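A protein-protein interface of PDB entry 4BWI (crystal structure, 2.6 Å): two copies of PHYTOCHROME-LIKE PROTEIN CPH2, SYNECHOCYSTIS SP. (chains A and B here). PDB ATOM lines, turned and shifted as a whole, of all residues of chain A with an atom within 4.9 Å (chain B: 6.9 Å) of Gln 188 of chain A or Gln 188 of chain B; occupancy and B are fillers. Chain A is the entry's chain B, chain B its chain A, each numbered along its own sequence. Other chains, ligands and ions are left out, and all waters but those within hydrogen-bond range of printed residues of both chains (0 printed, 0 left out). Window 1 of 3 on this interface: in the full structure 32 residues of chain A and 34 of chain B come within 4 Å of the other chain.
The side-chain carboxylate (OE2) of Glu 181 of chain B is in hydrogen-bond range of a ring nitrogen (NE2) of His 19 of chain A, at 2.8 Å. NE2 of Gln 188 of chain A is in hydrogen-bond range of OE1 of Gln 188 of chain B (3.1 Å).
The side-chain amide nitrogen (NE2) of Gln 149 of chain B is in hydrogen-bond range of the side-chain hydroxyl (OG1) of Thr 187 of chain B (3.0 Å). The side-chain hydroxyl (OG1) of Thr 187 of chain B lies within hydrogen-bond range of the backbone carbonyl oxygen (O) of Ser 183 of chain B, at 2.9 Å.
Among the printed residues, merely in contact across the chains: Leu 191 of chain A with Glu 181 of chain B, Gln 188 of chain A with Leu 184 of chain B, Leu 184 of chain A with Gln 188 of chain B, Leu 184 of chain A with Thr 187 of chain B, Thr 187 of chain A with Leu 184 of chain B and Leu 191 of chain A with Leu 184 of chain B.
Printed residues of chain B within 4 Å of His 19 of chain A: Glu 181. Of the printed residues of chain B, Leu 184 of chain A touches Thr 187 and Gln 188. Of the printed residues of chain B, Gln 188 of chain A touches Leu 184 and Gln 188. Printed residues of chain A within 4 Å of Leu 184 of chain B: Thr 187, Gln 188 and Leu 191. Printed residues of chain A within 4 Å of Gln 188 of chain B: Leu 184 (3.7 Å) and Gln 188 (3.1 Å). The nearest printed residue of chain A that does not touch Glu 181 of chain B is Ser 192 of chain A (5.8 Å).
Printed residues of chain B that touch a printed residue of chain A: Glu 181, Leu 184, Thr 187 and Gln 188. Hydrophobic or aromatic side chains of chain B that line the printed part of chain A: Leu 184. Of the 10 printed residues of chain A, 5 touch a printed residue of chain B. Printed residues of chain A that touch a printed residue of chain B: His 19, Leu 184, Thr 187, Gln 188 and Leu 191. Hydrophobic or aromatic side chains of chain A within 4 Å of the printed part of chain B: His 19, Leu 184 and Leu 191. Among the printed residues, 8 pairs touch across the chains. Among the printed residues, no Asp or Glu carboxylate lies within 4 Å of a Lys or Arg side-chain nitrogen of the other chain.
Leu 184 of chain A touches Thr 187 of chain B, and with the chains exchanged Thr 187 of chain A touches Leu 184 of chain B. Leu 184 of chain A touches Gln 188 of chain B, and with the chains exchanged Gln 188 of chain A touches Leu 184 of chain B. Gln 188 of chain B touches its own counterpart, Gln 188 of chain A. Leu 191 of chain A touches Leu 184 of chain B, but with the chains exchanged Leu 184 of chain A does not touch Leu 191 of chain B (4.4 Å). 10 positions are printed for both chains.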
ATOM      1  N   HIS A  19      11.696  16.187   8.403  1.00  0.00           N
ATOM      2  CA  HIS A  19      11.224  17.551   8.170  1.00  0.00           C
ATOM      3  C   HIS A  19       9.963  17.926   8.945  1.00  0.00           C
ATOM      4  O   HIS A  19       9.160  18.735   8.479  1.00  0.00           O
ATOM      5  CB  HIS A  19      11.013  17.790   6.671  1.00  0.00           C
ATOM      6  CG  HIS A  19      12.276  17.732   5.871  1.00  0.00           C
ATOM      7  ND1 HIS A  19      13.485  18.178   6.359  1.00  0.00           N
ATOM      8  CD2 HIS A  19      12.521  17.271   4.623  1.00  0.00           C
ATOM      9  CE1 HIS A  19      14.420  18.001   5.443  1.00  0.00           C
ATOM     10  NE2 HIS A  19      13.862  17.451   4.379  1.00  0.00           N
ATOM     11  N   LEU A 184      21.584  26.513   9.700  1.00  0.00           N
ATOM     12  CA  LEU A 184      21.070  25.148   9.705  1.00  0.00           C
ATOM     13  C   LEU A 184      19.589  25.132   9.349  1.00  0.00           C
ATOM     14  O   LEU A 184      19.145  24.316   8.544  1.00  0.00           O
ATOM     15  CB  LEU A 184      21.289  24.492  11.071  1.00  0.00           C
ATOM     16  CG  LEU A 184      20.778  23.056  11.230  1.00  0.00           C
ATOM     17  CD1 LEU A 184      21.562  22.090  10.351  1.00  0.00           C
ATOM     18  CD2 LEU A 184      20.829  22.623  12.685  1.00  0.00           C
ATOM     19  N   ALA A 185      18.831  26.042   9.947  1.00  0.00           N
ATOM     20  CA  ALA A 185      17.395  26.127   9.703  1.00  0.00           C
ATOM     21  C   ALA A 185      17.087  26.492   8.254  1.00  0.00           C
ATOM     22  O   ALA A 185      16.053  26.102   7.717  1.00  0.00           O
ATOM     23  CB  ALA A 185      16.755  27.129  10.653  1.00  0.00           C
ATOM     24  N   ILE A 186      17.984  27.245   7.626  1.00  0.00           N
ATOM     25  CA  ILE A 186      17.809  27.618   6.227  1.00  0.00           C
ATOM     26  C   ILE A 186      17.976  26.400   5.330  1.00  0.00           C
ATOM     27  O   ILE A 186      17.178  26.177   4.421  1.00  0.00           O
ATOM     28  CB  ILE A 186      18.812  28.703   5.792  1.00  0.00           C
ATOM     29  CG1 ILE A 186      18.615  29.975   6.618  1.00  0.00           C
ATOM     30  CG2 ILE A 186      18.653  29.012   4.315  1.00  0.00           C
ATOM     31  CD1 ILE A 186      19.708  30.992   6.424  1.00  0.00           C
ATOM     32  N   THR A 187      19.016  25.614   5.597  1.00  0.00           N
ATOM     33  CA  THR A 187      19.273  24.399   4.834  1.00  0.00           C
ATOM     34  C   THR A 187      18.117  23.415   4.967  1.00  0.00           C
ATOM     35  O   THR A 187      17.632  22.887   3.968  1.00  0.00           O
ATOM     36  CB  THR A 187      20.581  23.715   5.271  1.00  0.00           C
ATOM     37  OG1 THR A 187      21.670  24.635   5.125  1.00  0.00           O
ATOM     38  CG2 THR A 187      20.847  22.475   4.417  1.00  0.00           C
ATOM     39  N   GLN A 188      17.682  23.181   6.204  1.00  0.00           N
ATOM     40  CA  GLN A 188      16.538  22.314   6.476  1.00  0.00           C
ATOM     41  C   GLN A 188      15.302  22.788   5.717  1.00  0.00           C
ATOM     42  O   GLN A 188      14.567  21.984   5.144  1.00  0.00           O
ATOM     43  CB  GLN A 188      16.234  22.274   7.974  1.00  0.00           C
ATOM     44  CG  GLN A 188      17.316  21.639   8.830  1.00  0.00           C
ATOM     45  CD  GLN A 188      17.143  21.942  10.312  1.00  0.00           C
ATOM     46  OE1 GLN A 188      16.344  22.798  10.694  1.00  0.00           O
ATOM     47  NE2 GLN A 188      17.897  21.244  11.153  1.00  0.00           N
ATOM     48  N   SER A 189      15.086  24.100   5.711  1.00  0.00           N
ATOM     49  CA  SER A 189      13.948  24.701   5.021  1.00  0.00           C
ATOM     50  C   SER A 189      14.005  24.493   3.508  1.00  0.00           C
ATOM     51  O   SER A 189      12.995  24.172   2.883  1.00  0.00           O
ATOM     52  CB  SER A 189      13.859  26.197   5.342  1.00  0.00           C
ATOM     53  OG  SER A 189      12.852  26.830   4.572  1.00  0.00           O
ATOM     54  N   GLN A 190      15.184  24.681   2.924  1.00  0.00           N
ATOM     55  CA  GLN A 190      15.354  24.537   1.481  1.00  0.00           C
ATOM     56  C   GLN A 190      15.211  23.081   1.052  1.00  0.00           C
ATOM     57  O   GLN A 190      14.562  22.779   0.049  1.00  0.00           O
ATOM     58  CB  GLN A 190      16.710  25.088   1.037  1.00  0.00           C
ATOM     59  CG  GLN A 190      16.830  26.600   1.145  1.00  0.00           C
ATOM     60  CD  GLN A 190      18.215  27.104   0.789  1.00  0.00           C
ATOM     61  OE1 GLN A 190      18.429  28.307   0.631  1.00  0.00           O
ATOM     62  NE2 GLN A 190      19.167  26.185   0.664  1.00  0.00           N
ATOM     63  N   LEU A 191      15.823  22.184   1.819  1.00  0.00           N
ATOM     64  CA  LEU A 191      15.742  20.759   1.538  1.00  0.00           C
ATOM     65  C   LEU A 191      14.302  20.279   1.684  1.00  0.00           C
ATOM     66  O   LEU A 191      13.841  19.423   0.930  1.00  0.00           O
ATOM     67  CB  LEU A 191      16.678  19.975   2.464  1.00  0.00           C
ATOM     68  CG  LEU A 191      16.796  18.470   2.216  1.00  0.00           C
ATOM     69  CD1 LEU A 191      17.098  18.191   0.754  1.00  0.00           C
ATOM     70  CD2 LEU A 191      17.875  17.876   3.106  1.00  0.00           C
ATOM     71  N   SER A 192      13.591  20.850   2.652  1.00  0.00           N
ATOM     72  CA  SER A 192      12.175  20.555   2.842  1.00  0.00           C
ATOM     73  C   SER A 192      11.350  21.040   1.654  1.00  0.00           C
ATOM     74  O   SER A 192      10.329  20.444   1.312  1.00  0.00           O
ATOM     75  CB  SER A 192      11.663  21.204   4.128  1.00  0.00           C
ATOM     76  OG  SER A 192      10.265  21.031   4.261  1.00  0.00           O
ATOM     77  N   PHE B  18      16.585  22.830  19.129  1.00  0.00           N
ATOM     78  CA  PHE B  18      17.225  22.691  17.824  1.00  0.00           C
ATOM     79  C   PHE B  18      18.021  21.398  17.656  1.00  0.00           C
ATOM     80  O   PHE B  18      18.410  21.044  16.543  1.00  0.00           O
ATOM     81  CB  PHE B  18      18.130  23.894  17.545  1.00  0.00           C
ATOM     82  CG  PHE B  18      17.409  25.211  17.572  1.00  0.00           C
ATOM     83  CD1 PHE B  18      16.087  25.301  17.162  1.00  0.00           C
ATOM     84  CD2 PHE B  18      18.049  26.357  18.012  1.00  0.00           C
ATOM     85  CE1 PHE B  18      15.419  26.509  17.189  1.00  0.00           C
ATOM     86  CE2 PHE B  18      17.386  27.567  18.041  1.00  0.00           C
ATOM     87  CZ  PHE B  18      16.069  27.644  17.628  1.00  0.00           C
ATOM     88  N   HIS B  19      18.266  20.695  18.757  1.00  0.00           N
ATOM     89  CA  HIS B  19      19.073  19.482  18.702  1.00  0.00           C
ATOM     90  C   HIS B  19      18.420  18.307  19.419  1.00  0.00           C
ATOM     91  O   HIS B  19      19.073  17.304  19.710  1.00  0.00           O
ATOM     92  CB  HIS B  19      20.473  19.745  19.261  1.00  0.00           C
ATOM     93  CG  HIS B  19      21.230  20.793  18.508  1.00  0.00           C
ATOM     94  ND1 HIS B  19      21.502  20.690  17.161  1.00  0.00           N
ATOM     95  CD2 HIS B  19      21.770  21.968  18.911  1.00  0.00           C
ATOM     96  CE1 HIS B  19      22.178  21.754  16.767  1.00  0.00           C
ATOM     97  NE2 HIS B  19      22.355  22.545  17.810  1.00  0.00           N
ATOM     98  N   ALA B  21      16.892  15.700  18.595  1.00  0.00           N
ATOM     99  CA  ALA B  21      16.613  14.783  17.499  1.00  0.00           C
ATOM    100  C   ALA B  21      17.225  13.413  17.763  1.00  0.00           C
ATOM    101  O   ALA B  21      17.374  12.996  18.913  1.00  0.00           O
ATOM    102  CB  ALA B  21      17.137  15.352  16.189  1.00  0.00           C
ATOM    103  N   LEU B  22      17.573  12.718  16.686  1.00  0.00           N
ATOM    104  CA  LEU B  22      18.225  11.419  16.781  1.00  0.00           C
ATOM    105  C   LEU B  22      19.731  11.612  16.650  1.00  0.00           C
ATOM    106  O   LEU B  22      20.188  12.670  16.222  1.00  0.00           O
ATOM    107  CB  LEU B  22      17.718  10.481  15.681  1.00  0.00           C
ATOM    108  CG  LEU B  22      16.310   9.881  15.777  1.00  0.00           C
ATOM    109  CD1 LEU B  22      15.216  10.928  15.606  1.00  0.00           C
ATOM    110  CD2 LEU B  22      16.145   8.778  14.748  1.00  0.00           C
ATOM    111  N   THR B  27      20.569   8.107  12.472  1.00  0.00           N
ATOM    112  CA  THR B  27      20.012   8.751  11.287  1.00  0.00           C
ATOM    113  C   THR B  27      20.553   8.106  10.008  1.00  0.00           C
ATOM    114  O   THR B  27      19.810   7.884   9.053  1.00  0.00           O
ATOM    115  CB  THR B  27      20.292  10.270  11.281  1.00  0.00           C
ATOM    116  OG1 THR B  27      19.632  10.880  12.397  1.00  0.00           O
ATOM    117  CG2 THR B  27      19.789  10.908   9.996  1.00  0.00           C
ATOM    118  N   GLN B 149      30.259  17.734   2.567  1.00  0.00           N
ATOM    119  CA  GLN B 149      30.279  18.517   3.795  1.00  0.00           C
ATOM    120  C   GLN B 149      31.408  19.540   3.716  1.00  0.00           C
ATOM    121  O   GLN B 149      32.569  19.174   3.522  1.00  0.00           O
ATOM    122  CB  GLN B 149      30.464  17.614   5.017  1.00  0.00           C
ATOM    123  CG  GLN B 149      30.244  18.319   6.349  1.00  0.00           C
ATOM    124  CD  GLN B 149      28.780  18.633   6.616  1.00  0.00           C
ATOM    125  OE1 GLN B 149      27.885  18.000   6.061  1.00  0.00           O
ATOM    126  NE2 GLN B 149      28.534  19.614   7.478  1.00  0.00           N
ATOM    127  N   GLU B 181      20.294  14.822   2.712  1.00  0.00           N
ATOM    128  CA  GLU B 181      19.772  14.500   4.037  1.00  0.00           C
ATOM    129  C   GLU B 181      20.886  14.061   4.977  1.00  0.00           C
ATOM    130  O   GLU B 181      20.882  14.407   6.156  1.00  0.00           O
ATOM    131  CB  GLU B 181      18.698  13.412   3.956  1.00  0.00           C
ATOM    132  CG  GLU B 181      17.397  13.851   3.300  1.00  0.00           C
ATOM    133  CD  GLU B 181      16.613  14.848   4.140  1.00  0.00           C
ATOM    134  OE1 GLU B 181      16.903  14.988   5.347  1.00  0.00           O
ATOM    135  OE2 GLU B 181      15.703  15.498   3.588  1.00  0.00           O
ATOM    136  N   VAL B 182      21.832  13.291   4.447  1.00  0.00           N
ATOM    137  CA  VAL B 182      23.004  12.876   5.212  1.00  0.00           C
ATOM    138  C   VAL B 182      23.856  14.101   5.551  1.00  0.00           C
ATOM    139  O   VAL B 182      24.283  14.277   6.690  1.00  0.00           O
ATOM    140  CB  VAL B 182      23.852  11.842   4.438  1.00  0.00           C
ATOM    141  CG1 VAL B 182      25.145  11.546   5.175  1.00  0.00           C
ATOM    142  CG2 VAL B 182      23.065  10.565   4.221  1.00  0.00           C
ATOM    143  N   SER B 183      24.089  14.945   4.550  1.00  0.00           N
ATOM    144  CA  SER B 183      24.805  16.198   4.747  1.00  0.00           C
ATOM    145  C   SER B 183      24.120  17.057   5.806  1.00  0.00           C
ATOM    146  O   SER B 183      24.780  17.649   6.655  1.00  0.00           O
ATOM    147  CB  SER B 183      24.902  16.966   3.433  1.00  0.00           C
ATOM    148  OG  SER B 183      25.742  16.291   2.520  1.00  0.00           O
ATOM    149  N   LEU B 184      22.794  17.110   5.747  1.00  0.00           N
ATOM    150  CA  LEU B 184      22.018  17.854   6.727  1.00  0.00           C
ATOM    151  C   LEU B 184      22.257  17.314   8.133  1.00  0.00           C
ATOM    152  O   LEU B 184      22.485  18.079   9.069  1.00  0.00           O
ATOM    153  CB  LEU B 184      20.528  17.799   6.391  1.00  0.00           C
ATOM    154  CG  LEU B 184      19.646  18.662   7.296  1.00  0.00           C
ATOM    155  CD1 LEU B 184      20.067  20.116   7.182  1.00  0.00           C
ATOM    156  CD2 LEU B 184      18.175  18.496   6.960  1.00  0.00           C
ATOM    157  N   ALA B 185      22.218  15.992   8.273  1.00  0.00           N
ATOM    158  CA  ALA B 185      22.398  15.355   9.573  1.00  0.00           C
ATOM    159  C   ALA B 185      23.805  15.563  10.132  1.00  0.00           C
ATOM    160  O   ALA B 185      23.982  15.735  11.336  1.00  0.00           O
ATOM    161  CB  ALA B 185      22.075  13.870   9.484  1.00  0.00           C
ATOM    162  N   ILE B 186      24.799  15.536   9.252  1.00  0.00           N
ATOM    163  CA  ILE B 186      26.188  15.744   9.648  1.00  0.00           C
ATOM    164  C   ILE B 186      26.380  17.159  10.179  1.00  0.00           C
ATOM    165  O   ILE B 186      27.068  17.374  11.179  1.00  0.00           O
ATOM    166  CB  ILE B 186      27.143  15.484   8.468  1.00  0.00           C
ATOM    167  CG1 ILE B 186      27.139  13.994   8.116  1.00  0.00           C
ATOM    168  CG2 ILE B 186      28.554  15.941   8.797  1.00  0.00           C
ATOM    169  CD1 ILE B 186      27.718  13.693   6.759  1.00  0.00           C
ATOM    170  N   THR B 187      25.754  18.118   9.505  1.00  0.00           N
ATOM    171  CA  THR B 187      25.757  19.500   9.947  1.00  0.00           C
ATOM    172  C   THR B 187      25.073  19.603  11.302  1.00  0.00           C
ATOM    173  O   THR B 187      25.589  20.242  12.219  1.00  0.00           O
ATOM    174  CB  THR B 187      25.029  20.404   8.944  1.00  0.00           C
ATOM    175  OG1 THR B 187      25.635  20.263   7.654  1.00  0.00           O
ATOM    176  CG2 THR B 187      25.095  21.862   9.385  1.00  0.00           C
ATOM    177  N   GLN B 188      23.915  18.960  11.420  1.00  0.00           N
ATOM    178  CA  GLN B 188      23.160  18.949  12.670  1.00  0.00           C
ATOM    179  C   GLN B 188      24.006  18.405  13.814  1.00  0.00           C
ATOM    180  O   GLN B 188      24.106  19.027  14.874  1.00  0.00           O
ATOM    181  CB  GLN B 188      21.885  18.116  12.529  1.00  0.00           C
ATOM    182  CG  GLN B 188      20.804  18.753  11.669  1.00  0.00           C
ATOM    183  CD  GLN B 188      19.608  17.842  11.459  1.00  0.00           C
ATOM    184  OE1 GLN B 188      18.594  18.249  10.893  1.00  0.00           O
ATOM    185  NE2 GLN B 188      19.722  16.599  11.914  1.00  0.00           N
ATOM    186  N   SER B 189      24.622  17.246  13.586  1.00  0.00           N
ATOM    187  CA  SER B 189      25.428  16.567  14.597  1.00  0.00           C
ATOM    188  C   SER B 189      26.687  17.342  14.985  1.00  0.00           C
ATOM    189  O   SER B 189      27.080  17.358  16.152  1.00  0.00           O
ATOM    190  CB  SER B 189      25.806  15.160  14.120  1.00  0.00           C
ATOM    191  OG  SER B 189      26.558  14.467  15.101  1.00  0.00           O
ATOM    192  N   GLN B 190      27.317  17.981  14.005  1.00  0.00           N
ATOM    193  CA  GLN B 190      28.531  18.752  14.256  1.00  0.00           C
ATOM    194  C   GLN B 190      28.247  20.014  15.072  1.00  0.00           C
ATOM    195  O   GLN B 190      29.061  20.426  15.899  1.00  0.00           O
ATOM    196  CB  GLN B 190      29.221  19.117  12.938  1.00  0.00           C
ATOM    197  N   LEU B 191      27.091  20.627  14.840  1.00  0.00           N
ATOM    198  CA  LEU B 191      26.715  21.831  15.572  1.00  0.00           C
ATOM    199  C   LEU B 191      26.268  21.493  16.994  1.00  0.00           C
ATOM    200  O   LEU B 191      26.597  22.204  17.944  1.00  0.00           O
ATOM    201  CB  LEU B 191      25.621  22.607  14.832  1.00  0.00           C
ATOM    202  CG  LEU B 191      25.210  23.940  15.465  1.00  0.00           C
ATOM    203  CD1 LEU B 191      26.432  24.808  15.738  1.00  0.00           C
ATOM    204  CD2 LEU B 191      24.222  24.674  14.574  1.00  0.00           C
ATOM    205  N   SER B 192      25.525  20.398  17.133  1.00  0.00           N
ATOM    206  CA  SER B 192      25.084  19.935  18.443  1.00  0.00           C
ATOM    207  C   SER B 192      26.288  19.562  19.299  1.00  0.00           C
ATOM    208  O   SER B 192      26.262  19.690  20.522  1.00  0.00           O
ATOM    209  CB  SER B 192      24.142  18.739  18.303  1.00  0.00           C
ATOM    210  OG  SER B 192      23.718  18.280  19.575  1.00  0.00           O
ATOM    211  N   ARG B 193      27.345  19.100  18.640  1.00  0.00           N
ATOM    212  CA  ARG B 193      28.596  18.795  19.316  1.00  0.00           C
ATOM    213  C   ARG B 193      29.221  20.069  19.884  1.00  0.00           C
ATOM    214  O   ARG B 193      29.710  20.082  21.012  1.00  0.00           O
ATOM    215  CB  ARG B 193      29.564  18.122  18.343  1.00  0.00           C
ATOM    216  CG  ARG B 193      30.883  17.694  18.962  1.00  0.00           C
ATOM    217  CD  ARG B 193      31.708  16.880  17.976  1.00  0.00           C
ATOM    218  NE  ARG B 193      30.893  15.874  17.298  1.00  0.00           N
ATOM    219  CZ  ARG B 193      30.587  14.686  17.812  1.00  0.00           C
ATOM    220  NH1 ARG B 193      31.026  14.348  19.016  1.00  0.00           N
ATOM    221  NH2 ARG B 193      29.838  13.836  17.121  1.00  0.00           N
